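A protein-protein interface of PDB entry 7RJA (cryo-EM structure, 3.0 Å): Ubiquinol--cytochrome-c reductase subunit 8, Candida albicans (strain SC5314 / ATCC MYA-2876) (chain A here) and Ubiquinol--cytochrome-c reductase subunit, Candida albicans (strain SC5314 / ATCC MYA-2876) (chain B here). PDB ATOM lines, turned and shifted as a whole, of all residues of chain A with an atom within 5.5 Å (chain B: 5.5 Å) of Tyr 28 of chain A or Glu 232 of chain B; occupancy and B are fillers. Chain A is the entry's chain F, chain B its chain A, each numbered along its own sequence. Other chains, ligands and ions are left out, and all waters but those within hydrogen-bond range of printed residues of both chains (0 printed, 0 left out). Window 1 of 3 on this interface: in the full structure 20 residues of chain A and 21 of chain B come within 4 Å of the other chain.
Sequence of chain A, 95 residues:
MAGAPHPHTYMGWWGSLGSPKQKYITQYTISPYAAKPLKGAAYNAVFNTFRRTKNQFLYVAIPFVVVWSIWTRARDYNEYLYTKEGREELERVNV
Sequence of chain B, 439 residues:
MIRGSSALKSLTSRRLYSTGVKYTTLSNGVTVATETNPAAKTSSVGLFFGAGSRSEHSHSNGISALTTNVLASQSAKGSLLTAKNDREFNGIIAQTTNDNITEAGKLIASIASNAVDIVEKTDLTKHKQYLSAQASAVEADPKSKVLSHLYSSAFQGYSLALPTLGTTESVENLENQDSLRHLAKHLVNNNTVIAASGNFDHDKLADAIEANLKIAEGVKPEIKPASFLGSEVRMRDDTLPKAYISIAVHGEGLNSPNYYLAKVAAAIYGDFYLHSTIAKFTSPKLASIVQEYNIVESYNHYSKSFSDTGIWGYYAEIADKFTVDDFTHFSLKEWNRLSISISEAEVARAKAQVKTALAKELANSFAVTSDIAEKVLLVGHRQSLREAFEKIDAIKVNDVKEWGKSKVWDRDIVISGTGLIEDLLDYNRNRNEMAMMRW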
ATOM      1  N   THR A  26     -18.099 -23.229 -35.276  1.00  0.00           N
ATOM      2  CA  THR A  26     -17.278 -22.106 -34.842  1.00  0.00           C
ATOM      3  C   THR A  26     -18.202 -20.993 -34.373  1.00  0.00           C
ATOM      4  O   THR A  26     -19.106 -20.588 -35.109  1.00  0.00           O
ATOM      5  CB  THR A  26     -16.384 -21.612 -35.976  1.00  0.00           C
ATOM      6  OG1 THR A  26     -15.549 -22.683 -36.427  1.00  0.00           O
ATOM      7  CG2 THR A  26     -15.512 -20.473 -35.503  1.00  0.00           C
ATOM      8  N   GLN A  27     -17.980 -20.501 -33.157  1.00  0.00           N
ATOM      9  CA  GLN A  27     -18.821 -19.469 -32.559  1.00  0.00           C
ATOM     10  C   GLN A  27     -18.024 -18.175 -32.474  1.00  0.00           C
ATOM     11  O   GLN A  27     -17.087 -18.071 -31.678  1.00  0.00           O
ATOM     12  CB  GLN A  27     -19.308 -19.891 -31.176  1.00  0.00           C
ATOM     13  CG  GLN A  27     -19.944 -21.263 -31.134  1.00  0.00           C
ATOM     14  CD  GLN A  27     -20.396 -21.649 -29.747  1.00  0.00           C
ATOM     15  OE1 GLN A  27     -20.740 -20.791 -28.935  1.00  0.00           O
ATOM     16  NE2 GLN A  27     -20.410 -22.946 -29.468  1.00  0.00           N
ATOM     17  N   TYR A  28     -18.399 -17.192 -33.281  1.00  0.00           N
ATOM     18  CA  TYR A  28     -17.773 -15.882 -33.227  1.00  0.00           C
ATOM     19  C   TYR A  28     -18.614 -14.935 -32.384  1.00  0.00           C
ATOM     20  O   TYR A  28     -19.842 -15.034 -32.345  1.00  0.00           O
ATOM     21  CB  TYR A  28     -17.606 -15.292 -34.625  1.00  0.00           C
ATOM     22  CG  TYR A  28     -17.008 -16.236 -35.632  1.00  0.00           C
ATOM     23  CD1 TYR A  28     -15.647 -16.475 -35.660  1.00  0.00           C
ATOM     24  CD2 TYR A  28     -17.799 -16.857 -36.580  1.00  0.00           C
ATOM     25  CE1 TYR A  28     -15.097 -17.332 -36.582  1.00  0.00           C
ATOM     26  CE2 TYR A  28     -17.256 -17.709 -37.510  1.00  0.00           C
ATOM     27  CZ  TYR A  28     -15.904 -17.941 -37.508  1.00  0.00           C
ATOM     28  OH  TYR A  28     -15.354 -18.793 -38.433  1.00  0.00           O
ATOM     29  N   THR A  29     -17.940 -14.014 -31.706  1.00  0.00           N
ATOM     30  CA  THR A  29     -18.626 -12.957 -30.976  1.00  0.00           C
ATOM     31  C   THR A  29     -17.652 -11.812 -30.759  1.00  0.00           C
ATOM     32  O   THR A  29     -16.436 -11.979 -30.850  1.00  0.00           O
ATOM     33  CB  THR A  29     -19.179 -13.458 -29.642  1.00  0.00           C
ATOM     34  OG1 THR A  29     -19.885 -12.397 -28.990  1.00  0.00           O
ATOM     35  CG2 THR A  29     -18.065 -13.934 -28.748  1.00  0.00           C
ATOM     36  N   ILE A  30     -18.206 -10.641 -30.470  1.00  0.00           N
ATOM     37  CA  ILE A  30     -17.416  -9.455 -30.201  1.00  0.00           C
ATOM     38  C   ILE A  30     -17.583  -9.089 -28.733  1.00  0.00           C
ATOM     39  O   ILE A  30     -18.565  -9.447 -28.085  1.00  0.00           O
ATOM     40  CB  ILE A  30     -17.804  -8.278 -31.112  1.00  0.00           C
ATOM     41  CG1 ILE A  30     -19.288  -7.943 -30.949  1.00  0.00           C
ATOM     42  CG2 ILE A  30     -17.494  -8.610 -32.554  1.00  0.00           C
ATOM     43  CD1 ILE A  30     -19.740  -6.769 -31.781  1.00  0.00           C
ATOM     44  N   SER B 153      -9.394 -13.279 -35.510  1.00  0.00           N
ATOM     45  CA  SER B 153     -10.515 -12.655 -34.815  1.00  0.00           C
ATOM     46  C   SER B 153     -10.119 -11.309 -34.228  1.00  0.00           C
ATOM     47  O   SER B 153     -10.922 -10.371 -34.217  1.00  0.00           O
ATOM     48  CB  SER B 153     -11.033 -13.574 -33.714  1.00  0.00           C
ATOM     49  OG  SER B 153     -10.070 -13.718 -32.690  1.00  0.00           O
ATOM     50  N   GLY B 230     -11.594  -6.730 -29.576  1.00  0.00           N
ATOM     51  CA  GLY B 230     -11.842  -7.787 -28.620  1.00  0.00           C
ATOM     52  C   GLY B 230     -12.940  -8.706 -29.102  1.00  0.00           C
ATOM     53  O   GLY B 230     -14.039  -8.250 -29.420  1.00  0.00           O
ATOM     54  N   SER B 231     -12.657 -10.001 -29.164  1.00  0.00           N
ATOM     55  CA  SER B 231     -13.598 -10.955 -29.729  1.00  0.00           C
ATOM     56  C   SER B 231     -13.261 -12.335 -29.196  1.00  0.00           C
ATOM     57  O   SER B 231     -12.222 -12.545 -28.571  1.00  0.00           O
ATOM     58  CB  SER B 231     -13.552 -10.935 -31.256  1.00  0.00           C
ATOM     59  OG  SER B 231     -12.310 -11.420 -31.726  1.00  0.00           O
ATOM     60  N   GLU B 232     -14.157 -13.279 -29.449  1.00  0.00           N
ATOM     61  CA  GLU B 232     -13.961 -14.660 -29.044  1.00  0.00           C
ATOM     62  C   GLU B 232     -14.332 -15.573 -30.199  1.00  0.00           C
ATOM     63  O   GLU B 232     -15.344 -15.358 -30.870  1.00  0.00           O
ATOM     64  CB  GLU B 232     -14.793 -14.990 -27.804  1.00  0.00           C
ATOM     65  CG  GLU B 232     -14.710 -16.432 -27.342  1.00  0.00           C
ATOM     66  CD  GLU B 232     -15.919 -16.847 -26.535  1.00  0.00           C
ATOM     67  OE1 GLU B 232     -17.047 -16.739 -27.059  1.00  0.00           O
ATOM     68  OE2 GLU B 232     -15.743 -17.294 -25.382  1.00  0.00           O
ATOM     69  N   VAL B 233     -13.502 -16.585 -30.429  1.00  0.00           N
ATOM     70  CA  VAL B 233     -13.740 -17.594 -31.452  1.00  0.00           C
ATOM     71  C   VAL B 233     -13.547 -18.959 -30.810  1.00  0.00           C
ATOM     72  O   VAL B 233     -12.556 -19.182 -30.107  1.00  0.00           O
ATOM     73  CB  VAL B 233     -12.801 -17.415 -32.658  1.00  0.00           C
ATOM     74  CG1 VAL B 233     -11.364 -17.653 -32.255  1.00  0.00           C
ATOM     75  CG2 VAL B 233     -13.203 -18.339 -33.780  1.00  0.00           C
ATOM     76  N   ARG B 234     -14.490 -19.869 -31.041  1.00  0.00           N
ATOM     77  CA  ARG B 234     -14.508 -21.170 -30.373  1.00  0.00           C
ATOM     78  C   ARG B 234     -14.719 -22.261 -31.417  1.00  0.00           C
ATOM     79  O   ARG B 234     -15.839 -22.454 -31.895  1.00  0.00           O
ATOM     80  CB  ARG B 234     -15.603 -21.221 -29.318  1.00  0.00           C
ATOM     81  CG  ARG B 234     -15.517 -20.145 -28.260  1.00  0.00           C
ATOM     82  CD  ARG B 234     -16.837 -20.022 -27.528  1.00  0.00           C
ATOM     83  NE  ARG B 234     -17.071 -21.142 -26.627  1.00  0.00           N
ATOM     84  CZ  ARG B 234     -16.875 -21.110 -25.315  1.00  0.00           C
ATOM     85  NH1 ARG B 234     -16.420 -20.027 -24.706  1.00  0.00           N
ATOM     86  NH2 ARG B 234     -17.144 -22.195 -24.595  1.00  0.00           N
ATOM     87  N   VAL B 414      -8.968 -10.901 -26.574  1.00  0.00           N
ATOM     88  CA  VAL B 414      -9.360 -11.776 -27.666  1.00  0.00           C
ATOM     89  C   VAL B 414      -9.039 -13.200 -27.244  1.00  0.00           C
ATOM     90  O   VAL B 414      -7.960 -13.462 -26.697  1.00  0.00           O
ATOM     91  CB  VAL B 414      -8.647 -11.408 -28.975  1.00  0.00           C
ATOM     92  CG1 VAL B 414      -7.146 -11.463 -28.802  1.00  0.00           C
ATOM     93  CG2 VAL B 414      -9.084 -12.336 -30.085  1.00  0.00           C
ATOM     94  N   ILE B 415      -9.976 -14.112 -27.489  1.00  0.00           N
ATOM     95  CA  ILE B 415      -9.901 -15.478 -26.997  1.00  0.00           C
ATOM     96  C   ILE B 415     -10.016 -16.437 -28.171  1.00  0.00           C
ATOM     97  O   ILE B 415     -10.624 -16.126 -29.199  1.00  0.00           O
ATOM     98  CB  ILE B 415     -11.007 -15.764 -25.957  1.00  0.00           C
ATOM     99  CG1 ILE B 415     -10.973 -14.719 -24.844  1.00  0.00           C
ATOM    100  CG2 ILE B 415     -10.851 -17.161 -25.385  1.00  0.00           C
ATOM    101  CD1 ILE B 415     -12.081 -14.867 -23.834  1.00  0.00           C
ATOM    102  N   SER B 416      -9.418 -17.614 -28.010  1.00  0.00           N
ATOM    103  CA  SER B 416      -9.514 -18.673 -29.000  1.00  0.00           C
ATOM    104  C   SER B 416      -9.447 -20.009 -28.281  1.00  0.00           C
ATOM    105  O   SER B 416      -8.808 -20.125 -27.235  1.00  0.00           O
ATOM    106  CB  SER B 416      -8.394 -18.576 -30.035  1.00  0.00           C
ATOM    107  OG  SER B 416      -8.424 -17.326 -30.693  1.00  0.00           O
ATOM    108  N   LEU B 424     -14.753 -23.539 -21.012  1.00  0.00           N
ATOM    109  CA  LEU B 424     -14.308 -22.168 -21.237  1.00  0.00           C
ATOM    110  C   LEU B 424     -15.529 -21.263 -21.214  1.00  0.00           C
ATOM    111  O   LEU B 424     -16.255 -21.153 -22.203  1.00  0.00           O
ATOM    112  CB  LEU B 424     -13.561 -22.057 -22.560  1.00  0.00           C
ATOM    113  CG  LEU B 424     -13.062 -20.659 -22.922  1.00  0.00           C
ATOM    114  CD1 LEU B 424     -12.002 -20.206 -21.945  1.00  0.00           C
ATOM    115  CD2 LEU B 424     -12.525 -20.632 -24.338  1.00  0.00           C
ATOM    116  N   LEU B 425     -15.760 -20.606 -20.082  1.00  0.00           N
ATOM    117  CA  LEU B 425     -16.932 -19.755 -19.944  1.00  0.00           C
ATOM    118  C   LEU B 425     -16.891 -18.636 -20.977  1.00  0.00           C
ATOM    119  O   LEU B 425     -15.825 -18.152 -21.363  1.00  0.00           O
ATOM    120  CB  LEU B 425     -17.000 -19.169 -18.534  1.00  0.00           C
ATOM    121  CG  LEU B 425     -17.580 -20.068 -17.440  1.00  0.00           C
ATOM    122  CD1 LEU B 425     -19.023 -20.412 -17.729  1.00  0.00           C
ATOM    123  CD2 LEU B 425     -16.761 -21.324 -17.295  1.00  0.00           C
ATOM    124  N   ASP B 426     -18.074 -18.221 -21.426  1.00  0.00           N
ATOM    125  CA  ASP B 426     -18.158 -17.257 -22.510  1.00  0.00           C
ATOM    126  C   ASP B 426     -17.452 -15.957 -22.137  1.00  0.00           C
ATOM    127  O   ASP B 426     -17.006 -15.755 -21.008  1.00  0.00           O
ATOM    128  CB  ASP B 426     -19.615 -16.984 -22.880  1.00  0.00           C
ATOM    129  CG  ASP B 426     -20.195 -18.052 -23.787  1.00  0.00           C
ATOM    130  OD1 ASP B 426     -19.430 -18.664 -24.560  1.00  0.00           O
ATOM    131  OD2 ASP B 426     -21.418 -18.278 -23.737  1.00  0.00           O
ATOM    132  N   TYR B 427     -17.352 -15.073 -23.131  1.00  0.00           N
ATOM    133  CA  TYR B 427     -16.521 -13.881 -23.031  1.00  0.00           C
ATOM    134  C   TYR B 427     -16.659 -13.163 -21.695  1.00  0.00           C
ATOM    135  O   TYR B 427     -15.670 -12.962 -20.985  1.00  0.00           O
ATOM    136  CB  TYR B 427     -16.863 -12.919 -24.167  1.00  0.00           C
ATOM    137  CG  TYR B 427     -15.749 -11.954 -24.440  1.00  0.00           C
ATOM    138  CD1 TYR B 427     -14.598 -12.365 -25.079  1.00  0.00           C
ATOM    139  CD2 TYR B 427     -15.826 -10.645 -24.013  1.00  0.00           C
ATOM    140  CE1 TYR B 427     -13.571 -11.493 -25.317  1.00  0.00           C
ATOM    141  CE2 TYR B 427     -14.801  -9.769 -24.239  1.00  0.00           C
ATOM    142  CZ  TYR B 427     -13.677 -10.195 -24.894  1.00  0.00           C
ATOM    143  OH  TYR B 427     -12.644  -9.319 -25.127  1.00  0.00           O
ATOM    144  N   ASN B 430     -14.469 -14.077 -18.622  1.00  0.00           N
ATOM    145  CA  ASN B 430     -13.040 -13.816 -18.756  1.00  0.00           C
ATOM    146  C   ASN B 430     -12.759 -12.324 -18.832  1.00  0.00           C
ATOM    147  O   ASN B 430     -11.797 -11.833 -18.232  1.00  0.00           O
ATOM    148  CB  ASN B 430     -12.493 -14.530 -19.988  1.00  0.00           C
ATOM    149  CG  ASN B 430     -12.784 -16.013 -19.976  1.00  0.00           C
ATOM    150  OD1 ASN B 430     -13.287 -16.566 -20.950  1.00  0.00           O
ATOM    151  ND2 ASN B 430     -12.468 -16.667 -18.867  1.00  0.00           N
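Among the printed residues, merely in contact across the chains: Thr 29 of chain A with Ser 231 of chain B, Thr 26 of chain A with Arg 234 of chain B, Gln 27 of chain A with Val 233 of chain B, Tyr 28 of chain A with Glu 232 of chain B, Tyr 28 of chain A with Val 233 of chain B, Thr 26 of chain A with Val 233 of chain B and Ile 30 of chain A with Gly 230 of chain B.
Printed residues of chain A that touch a printed residue of chain B: Thr 26, Gln 27, Tyr 28, Thr 29 and Ile 30.
Hydrophobic or aromatic side chains of chain A within 4 Å of the printed part of chain B: Tyr 28.
Of the 14 printed residues of chain B, 5 touch a printed residue of chain A.
Hydrophobic or aromatic side chains of chain B that line the printed part of chain A: Val 233.
The backbone carbonyl oxygen (O) of Glu 232 of chain B lies close to the backbone carbonyl oxygen (O) of Gln 27 of chain A, at 3.3 Å.
O of Thr 29 of chain A sits at hydrogen-bond distance from N of Glu 232 of chain B, at 3.0 Å.
The backbone NH (N) of Gln 27 of chain A lies within hydrogen-bond range of the backbone carbonyl oxygen (O) of Arg 234 of chain B.
The guanidinium group of Arg 234 of chain B is in salt-bridge range of the side-chain carboxylate of Asp 426 of chain B.
The backbone carbonyl oxygen (O) of Leu 424 of chain B is in hydrogen-bond range of the guanidinium group (NH1) of Arg 234 of chain B (2.7 Å).
O of Ser 153 of chain B lies within hydrogen-bond range of OG of Ser 231 of chain B (3.0 Å).
The side-chain carboxylate (OE2) of Glu 232 of chain B is in salt-bridge range of the guanidinium group (NH1) of Arg 234 of chain B (2.9 Å).
The backbone carbonyl oxygen (O) of Ser 231 of chain B is in hydrogen-bond range of the backbone NH (N) of Ile 415 of chain B, at 2.9 Å.
N of Val 233 of chain B sits at hydrogen-bond distance from O of Ile 415 of chain B (3.2 Å).
Of chain A, only Gln 27, Tyr 28 and Thr 29 come within 4 Å of Glu 232 of chain B.
Of the printed residues of chain A, Gly 230 of chain B touches Ile 30 (3.7 Å).
Of the printed residues of chain B, Ile 30 of chain A touches Gly 230.
Printed residues of chain A within 4 Å of Ser 231 of chain B: Thr 29 (3.1 Å).
The nearest residue of chain A that does not touch Glu 232 of chain B is Ile 30 of chain A (4.9 Å).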
